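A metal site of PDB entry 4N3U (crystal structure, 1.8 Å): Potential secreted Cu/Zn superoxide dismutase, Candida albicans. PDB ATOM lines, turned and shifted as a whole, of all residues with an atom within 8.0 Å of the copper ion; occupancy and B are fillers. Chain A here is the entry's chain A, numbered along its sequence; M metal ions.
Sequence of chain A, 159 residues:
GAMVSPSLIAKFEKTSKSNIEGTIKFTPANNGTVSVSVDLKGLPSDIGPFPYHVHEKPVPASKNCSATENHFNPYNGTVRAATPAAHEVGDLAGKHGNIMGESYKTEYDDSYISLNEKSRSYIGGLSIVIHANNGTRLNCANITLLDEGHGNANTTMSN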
ATOM      1  N   PRO A  51      35.363  30.569 -26.312  1.00  0.00           N
ATOM      2  CA  PRO A  51      34.528  30.290 -25.142  1.00  0.00           C
ATOM      3  C   PRO A  51      34.269  28.787 -24.998  1.00  0.00           C
ATOM      4  O   PRO A  51      34.174  28.077 -25.997  1.00  0.00           O
ATOM      5  CB  PRO A  51      33.232  31.042 -25.441  1.00  0.00           C
ATOM      6  CG  PRO A  51      33.621  32.114 -26.435  1.00  0.00           C
ATOM      7  CD  PRO A  51      34.737  31.511 -27.248  1.00  0.00           C
ATOM      8  N   TYR A  52      34.201  28.306 -23.770  1.00  0.00           N
ATOM      9  CA  TYR A  52      33.839  26.913 -23.541  1.00  0.00           C
ATOM     10  C   TYR A  52      33.015  26.813 -22.275  1.00  0.00           C
ATOM     11  O   TYR A  52      33.273  27.537 -21.300  1.00  0.00           O
ATOM     12  CB  TYR A  52      35.078  26.009 -23.489  1.00  0.00           C
ATOM     13  CG  TYR A  52      36.005  26.242 -22.302  1.00  0.00           C
ATOM     14  CD1 TYR A  52      36.785  27.377 -22.223  1.00  0.00           C
ATOM     15  CD2 TYR A  52      36.114  25.302 -21.285  1.00  0.00           C
ATOM     16  CE1 TYR A  52      37.652  27.584 -21.163  1.00  0.00           C
ATOM     17  CE2 TYR A  52      36.958  25.504 -20.208  1.00  0.00           C
ATOM     18  CZ  TYR A  52      37.735  26.629 -20.147  1.00  0.00           C
ATOM     19  OH  TYR A  52      38.584  26.853 -19.092  1.00  0.00           O
ATOM     20  N   HIS A  53      32.019  25.932 -22.302  1.00  0.00           N
ATOM     21  CA  HIS A  53      31.023  25.865 -21.249  1.00  0.00           C
ATOM     22  C   HIS A  53      30.564  24.429 -21.038  1.00  0.00           C
ATOM     23  O   HIS A  53      30.648  23.607 -21.948  1.00  0.00           O
ATOM     24  CB  HIS A  53      29.796  26.729 -21.581  1.00  0.00           C
ATOM     25  CG  HIS A  53      30.098  27.970 -22.365  1.00  0.00           C
ATOM     26  ND1 HIS A  53      29.921  28.049 -23.730  1.00  0.00           N
ATOM     27  CD2 HIS A  53      30.534  29.186 -21.971  1.00  0.00           C
ATOM     28  CE1 HIS A  53      30.260  29.260 -24.148  1.00  0.00           C
ATOM     29  NE2 HIS A  53      30.629  29.969 -23.098  1.00  0.00           N
ATOM     30  N   VAL A  54      30.078  24.154 -19.835  1.00  0.00           N
ATOM     31  CA  VAL A  54      29.338  22.924 -19.573  1.00  0.00           C
ATOM     32  C   VAL A  54      27.932  23.074 -20.133  1.00  0.00           C
ATOM     33  O   VAL A  54      27.231  24.030 -19.796  1.00  0.00           O
ATOM     34  CB  VAL A  54      29.230  22.585 -18.060  1.00  0.00           C
ATOM     35  CG1 VAL A  54      28.523  21.261 -17.885  1.00  0.00           C
ATOM     36  CG2 VAL A  54      30.597  22.531 -17.432  1.00  0.00           C
ATOM     37  N   HIS A  55      27.526  22.149 -20.991  1.00  0.00           N
ATOM     38  CA  HIS A  55      26.177  22.176 -21.548  1.00  0.00           C
ATOM     39  C   HIS A  55      25.326  21.090 -20.907  1.00  0.00           C
ATOM     40  O   HIS A  55      25.845  20.225 -20.208  1.00  0.00           O
ATOM     41  CB  HIS A  55      26.231  22.007 -23.069  1.00  0.00           C
ATOM     42  CG  HIS A  55      26.673  23.239 -23.788  1.00  0.00           C
ATOM     43  ND1 HIS A  55      25.892  23.866 -24.736  1.00  0.00           N
ATOM     44  CD2 HIS A  55      27.804  23.972 -23.680  1.00  0.00           C
ATOM     45  CE1 HIS A  55      26.522  24.927 -25.190  1.00  0.00           C
ATOM     46  NE2 HIS A  55      27.692  25.017 -24.571  1.00  0.00           N
ATOM     47  N   CYS A  65      27.416  18.665 -31.856  1.00  0.00           N
ATOM     48  CA  CYS A  65      27.524  19.468 -30.635  1.00  0.00           C
ATOM     49  C   CYS A  65      26.275  20.303 -30.378  1.00  0.00           C
ATOM     50  O   CYS A  65      26.011  20.717 -29.242  1.00  0.00           O
ATOM     51  CB  CYS A  65      28.776  20.363 -30.689  1.00  0.00           C
ATOM     52  SG  CYS A  65      30.339  19.432 -30.836  1.00  0.00           S
ATOM     53  N   THR A  68      23.792  19.033 -27.555  1.00  0.00           N
ATOM     54  CA  THR A  68      24.048  19.208 -26.129  1.00  0.00           C
ATOM     55  C   THR A  68      23.135  20.291 -25.552  1.00  0.00           C
ATOM     56  O   THR A  68      23.106  20.518 -24.348  1.00  0.00           O
ATOM     57  CB  THR A  68      25.506  19.616 -25.867  1.00  0.00           C
ATOM     58  OG1 THR A  68      25.763  20.853 -26.526  1.00  0.00           O
ATOM     59  CG2 THR A  68      26.462  18.564 -26.382  1.00  0.00           C
ATOM     60  N   GLU A  69      22.401  20.957 -26.445  1.00  0.00           N
ATOM     61  CA  GLU A  69      21.467  22.039 -26.109  1.00  0.00           C
ATOM     62  C   GLU A  69      22.160  23.183 -25.363  1.00  0.00           C
ATOM     63  O   GLU A  69      23.249  23.588 -25.758  1.00  0.00           O
ATOM     64  CB  GLU A  69      20.277  21.480 -25.323  1.00  0.00           C
ATOM     65  CG  GLU A  69      19.393  20.568 -26.197  1.00  0.00           C
ATOM     66  CD  GLU A  69      18.275  19.872 -25.439  1.00  0.00           C
ATOM     67  OE1 GLU A  69      18.028  20.228 -24.262  1.00  0.00           O
ATOM     68  OE2 GLU A  69      17.647  18.964 -26.019  1.00  0.00           O
ATOM     69  N   ASN A  70      21.548  23.729 -24.323  1.00  0.00           N
ATOM     70  CA  ASN A  70      22.055  24.972 -23.733  1.00  0.00           C
ATOM     71  C   ASN A  70      23.042  24.777 -22.586  1.00  0.00           C
ATOM     72  O   ASN A  70      23.410  23.661 -22.241  1.00  0.00           O
ATOM     73  CB  ASN A  70      20.886  25.832 -23.234  1.00  0.00           C
ATOM     74  CG  ASN A  70      19.840  26.081 -24.313  1.00  0.00           C
ATOM     75  OD1 ASN A  70      20.168  26.451 -25.435  1.00  0.00           O
ATOM     76  ND2 ASN A  70      18.579  25.860 -23.967  1.00  0.00           N
ATOM     77  N   HIS A  71      23.456  25.899 -21.995  1.00  0.00           N
ATOM     78  CA  HIS A  71      24.382  25.876 -20.877  1.00  0.00           C
ATOM     79  C   HIS A  71      23.754  25.301 -19.612  1.00  0.00           C
ATOM     80  O   HIS A  71      22.559  25.451 -19.369  1.00  0.00           O
ATOM     81  CB  HIS A  71      24.911  27.280 -20.580  1.00  0.00           C
ATOM     82  CG  HIS A  71      25.752  27.838 -21.681  1.00  0.00           C
ATOM     83  ND1 HIS A  71      26.388  29.065 -21.595  1.00  0.00           N
ATOM     84  CD2 HIS A  71      26.051  27.346 -22.898  1.00  0.00           C
ATOM     85  CE1 HIS A  71      27.049  29.292 -22.709  1.00  0.00           C
ATOM     86  NE2 HIS A  71      26.860  28.261 -23.522  1.00  0.00           N
ATOM     87  N   PHE A  72      24.588  24.641 -18.822  1.00  0.00           N
ATOM     88  CA  PHE A  72      24.198  24.173 -17.497  1.00  0.00           C
ATOM     89  C   PHE A  72      24.151  25.390 -16.572  1.00  0.00           C
ATOM     90  O   PHE A  72      25.185  26.012 -16.307  1.00  0.00           O
ATOM     91  CB  PHE A  72      25.183  23.114 -17.004  1.00  0.00           C
ATOM     92  CG  PHE A  72      24.878  22.585 -15.636  1.00  0.00           C
ATOM     93  CD1 PHE A  72      23.677  21.947 -15.372  1.00  0.00           C
ATOM     94  CD2 PHE A  72      25.809  22.696 -14.624  1.00  0.00           C
ATOM     95  CE1 PHE A  72      23.411  21.429 -14.101  1.00  0.00           C
ATOM     96  CE2 PHE A  72      25.550  22.194 -13.362  1.00  0.00           C
ATOM     97  CZ  PHE A  72      24.342  21.562 -13.095  1.00  0.00           C
ATOM     98  N   GLU A  88      26.847  31.764 -14.856  1.00  0.00           N
ATOM     99  CA  GLU A  88      26.258  30.421 -14.893  1.00  0.00           C
ATOM    100  C   GLU A  88      27.278  29.408 -14.401  1.00  0.00           C
ATOM    101  O   GLU A  88      28.454  29.526 -14.732  1.00  0.00           O
ATOM    102  CB  GLU A  88      25.835  30.046 -16.317  1.00  0.00           C
ATOM    103  CG  GLU A  88      25.095  31.108 -17.099  1.00  0.00           C
ATOM    104  CD  GLU A  88      25.071  30.794 -18.585  1.00  0.00           C
ATOM    105  OE1 GLU A  88      24.051  31.089 -19.246  1.00  0.00           O
ATOM    106  OE2 GLU A  88      26.074  30.256 -19.087  1.00  0.00           O
ATOM    107  N   GLY A  90      27.918  26.494 -15.437  1.00  0.00           N
ATOM    108  CA  GLY A  90      28.606  25.953 -16.600  1.00  0.00           C
ATOM    109  C   GLY A  90      29.500  26.894 -17.385  1.00  0.00           C
ATOM    110  O   GLY A  90      30.222  26.441 -18.277  1.00  0.00           O
ATOM    111  N   ASP A  91      29.483  28.191 -17.083  1.00  0.00           N
ATOM    112  CA  ASP A  91      30.246  29.147 -17.877  1.00  0.00           C
ATOM    113  C   ASP A  91      31.697  29.229 -17.416  1.00  0.00           C
ATOM    114  O   ASP A  91      32.110  30.205 -16.796  1.00  0.00           O
ATOM    115  CB  ASP A  91      29.589  30.535 -17.824  1.00  0.00           C
ATOM    116  CG  ASP A  91      30.297  31.565 -18.700  1.00  0.00           C
ATOM    117  OD1 ASP A  91      31.181  31.200 -19.495  1.00  0.00           O
ATOM    118  OD2 ASP A  91      29.972  32.764 -18.575  1.00  0.00           O
ATOM    119  N   SER A 127      28.204  17.679 -20.615  1.00  0.00           N
ATOM    120  CA  SER A 127      29.154  17.797 -21.699  1.00  0.00           C
ATOM    121  C   SER A 127      29.850  19.160 -21.697  1.00  0.00           C
ATOM    122  O   SER A 127      29.388  20.101 -21.048  1.00  0.00           O
ATOM    123  CB  SER A 127      28.446  17.584 -23.044  1.00  0.00           C
ATOM    124  OG  SER A 127      27.436  18.562 -23.238  1.00  0.00           O
ATOM    125  N   ILE A 128      30.948  19.257 -22.424  1.00  0.00           N
ATOM    126  CA  ILE A 128      31.599  20.541 -22.622  1.00  0.00           C
ATOM    127  C   ILE A 128      31.629  20.838 -24.116  1.00  0.00           C
ATOM    128  O   ILE A 128      31.920  19.962 -24.923  1.00  0.00           O
ATOM    129  CB  ILE A 128      33.017  20.571 -22.045  1.00  0.00           C
ATOM    130  CG1 ILE A 128      32.966  20.262 -20.545  1.00  0.00           C
ATOM    131  CG2 ILE A 128      33.673  21.934 -22.295  1.00  0.00           C
ATOM    132  CD1 ILE A 128      34.330  20.037 -19.931  1.00  0.00           C
ATOM    133  N   VAL A 129      31.302  22.067 -24.473  1.00  0.00           N
ATOM    134  CA  VAL A 129      31.378  22.509 -25.861  1.00  0.00           C
ATOM    135  C   VAL A 129      32.402  23.609 -25.968  1.00  0.00           C
ATOM    136  O   VAL A 129      32.435  24.497 -25.113  1.00  0.00           O
ATOM    137  CB  VAL A 129      30.023  23.052 -26.379  1.00  0.00           C
ATOM    138  CG1 VAL A 129      30.182  23.617 -27.814  1.00  0.00           C
ATOM    139  CG2 VAL A 129      28.962  21.959 -26.349  1.00  0.00           C
ATOM    140  N   ILE A 130      33.247  23.555 -27.001  1.00  0.00           N
ATOM    141  CA  ILE A 130      34.193  24.634 -27.300  1.00  0.00           C
ATOM    142  C   ILE A 130      33.687  25.398 -28.521  1.00  0.00           C
ATOM    143  O   ILE A 130      33.388  24.792 -29.537  1.00  0.00           O
ATOM    144  CB  ILE A 130      35.612  24.096 -27.565  1.00  0.00           C
ATOM    145  CG1 ILE A 130      36.133  23.367 -26.315  1.00  0.00           C
ATOM    146  CG2 ILE A 130      36.579  25.210 -27.954  1.00  0.00           C
ATOM    147  CD1 ILE A 130      37.397  22.588 -26.573  1.00  0.00           C
ATOM    148  N   HIS A 131      33.579  26.722 -28.402  1.00  0.00           N
ATOM    149  CA  HIS A 131      33.045  27.554 -29.492  1.00  0.00           C
ATOM    150  C   HIS A 131      34.119  28.392 -30.153  1.00  0.00           C
ATOM    151  O   HIS A 131      35.093  28.789 -29.523  1.00  0.00           O
ATOM    152  CB  HIS A 131      31.972  28.530 -28.983  1.00  0.00           C
ATOM    153  CG  HIS A 131      30.885  27.905 -28.167  1.00  0.00           C
ATOM    154  ND1 HIS A 131      29.607  27.737 -28.644  1.00  0.00           N
ATOM    155  CD2 HIS A 131      30.880  27.468 -26.884  1.00  0.00           C
ATOM    156  CE1 HIS A 131      28.867  27.189 -27.700  1.00  0.00           C
ATOM    157  NE2 HIS A 131      29.608  27.024 -26.621  1.00  0.00           N
ATOM    158  N   GLY A 135      30.649  32.041 -31.787  1.00  0.00           N
ATOM    159  CA  GLY A 135      29.642  31.188 -31.185  1.00  0.00           C
ATOM    160  C   GLY A 135      29.505  29.830 -31.841  1.00  0.00           C
ATOM    161  O   GLY A 135      28.830  28.954 -31.302  1.00  0.00           O
ATOM    162  N   THR A 136      30.150  29.646 -32.982  1.00  0.00           N
ATOM    163  CA  THR A 136      30.028  28.369 -33.699  1.00  0.00           C
ATOM    164  C   THR A 136      30.566  27.226 -32.845  1.00  0.00           C
ATOM    165  O   THR A 136      31.646  27.354 -32.270  1.00  0.00           O
ATOM    166  CB  THR A 136      30.781  28.406 -35.035  1.00  0.00           C
ATOM    167  OG1 THR A 136      30.148  29.345 -35.900  1.00  0.00           O
ATOM    168  CG2 THR A 136      30.794  27.024 -35.682  1.00  0.00           C
ATOM    169  N   ARG A 137      29.830  26.125 -32.737  1.00  0.00           N
ATOM    170  CA  ARG A 137      30.298  25.014 -31.904  1.00  0.00           C
ATOM    171  C   ARG A 137      31.322  24.203 -32.692  1.00  0.00           C
ATOM    172  O   ARG A 137      31.032  23.684 -33.764  1.00  0.00           O
ATOM    173  CB  ARG A 137      29.113  24.168 -31.438  1.00  0.00           C
ATOM    174  CG  ARG A 137      28.071  25.015 -30.686  1.00  0.00           C
ATOM    175  CD  ARG A 137      26.919  24.221 -30.132  1.00  0.00           C
ATOM    176  NE  ARG A 137      25.983  25.088 -29.413  1.00  0.00           N
ATOM    177  CZ  ARG A 137      25.068  24.663 -28.539  1.00  0.00           C
ATOM    178  NH1 ARG A 137      24.971  23.370 -28.242  1.00  0.00           N
ATOM    179  NH2 ARG A 137      24.265  25.542 -27.950  1.00  0.00           N
HETATM  180 CU    CU M   1      28.808  26.732 -24.856  1.00  0.00          CU
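The copper ion is bound by NE2 of His 131 (2.0 Å), ND1 of His 53 (2.1 Å) and NE2 of His 55 (2.1 Å). The copper ion has three donor atoms within binding distance. Slightly farther from the copper ion lies NE2 of His 71 (2.8 Å).
Of the 22 residues printed, 4 come within 4 Å of the copper ion. The nearest printed residue that does not touch the copper ion is Val 129 (4.2 Å).
The backbone NH of His 55 sits at hydrogen-bond distance from the backbone carbonyl oxygen of Ser 127. The side-chain carboxylate of Glu 88 sits at hydrogen-bond distance from a ring nitrogen (ND1) of His 71 (2.8 Å). A ring nitrogen (ND1) of His 55 is in hydrogen-bond range of the backbone carbonyl oxygen (O) of Glu 69, at 2.8 Å. A ring nitrogen (ND1) of His 131 is in hydrogen-bond range of the backbone carbonyl oxygen (O) of Gly 135. The backbone carbonyl oxygen (O) of His 53 is in hydrogen-bond range of the backbone NH (N) of Val 129 (3.0 Å). A ring nitrogen (NE2) of His 71 sits close to a ring nitrogen (ND1) of His 53 (3.1 Å). N of His 131 sits at hydrogen-bond distance from O of Pro 51, at 2.8 Å.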
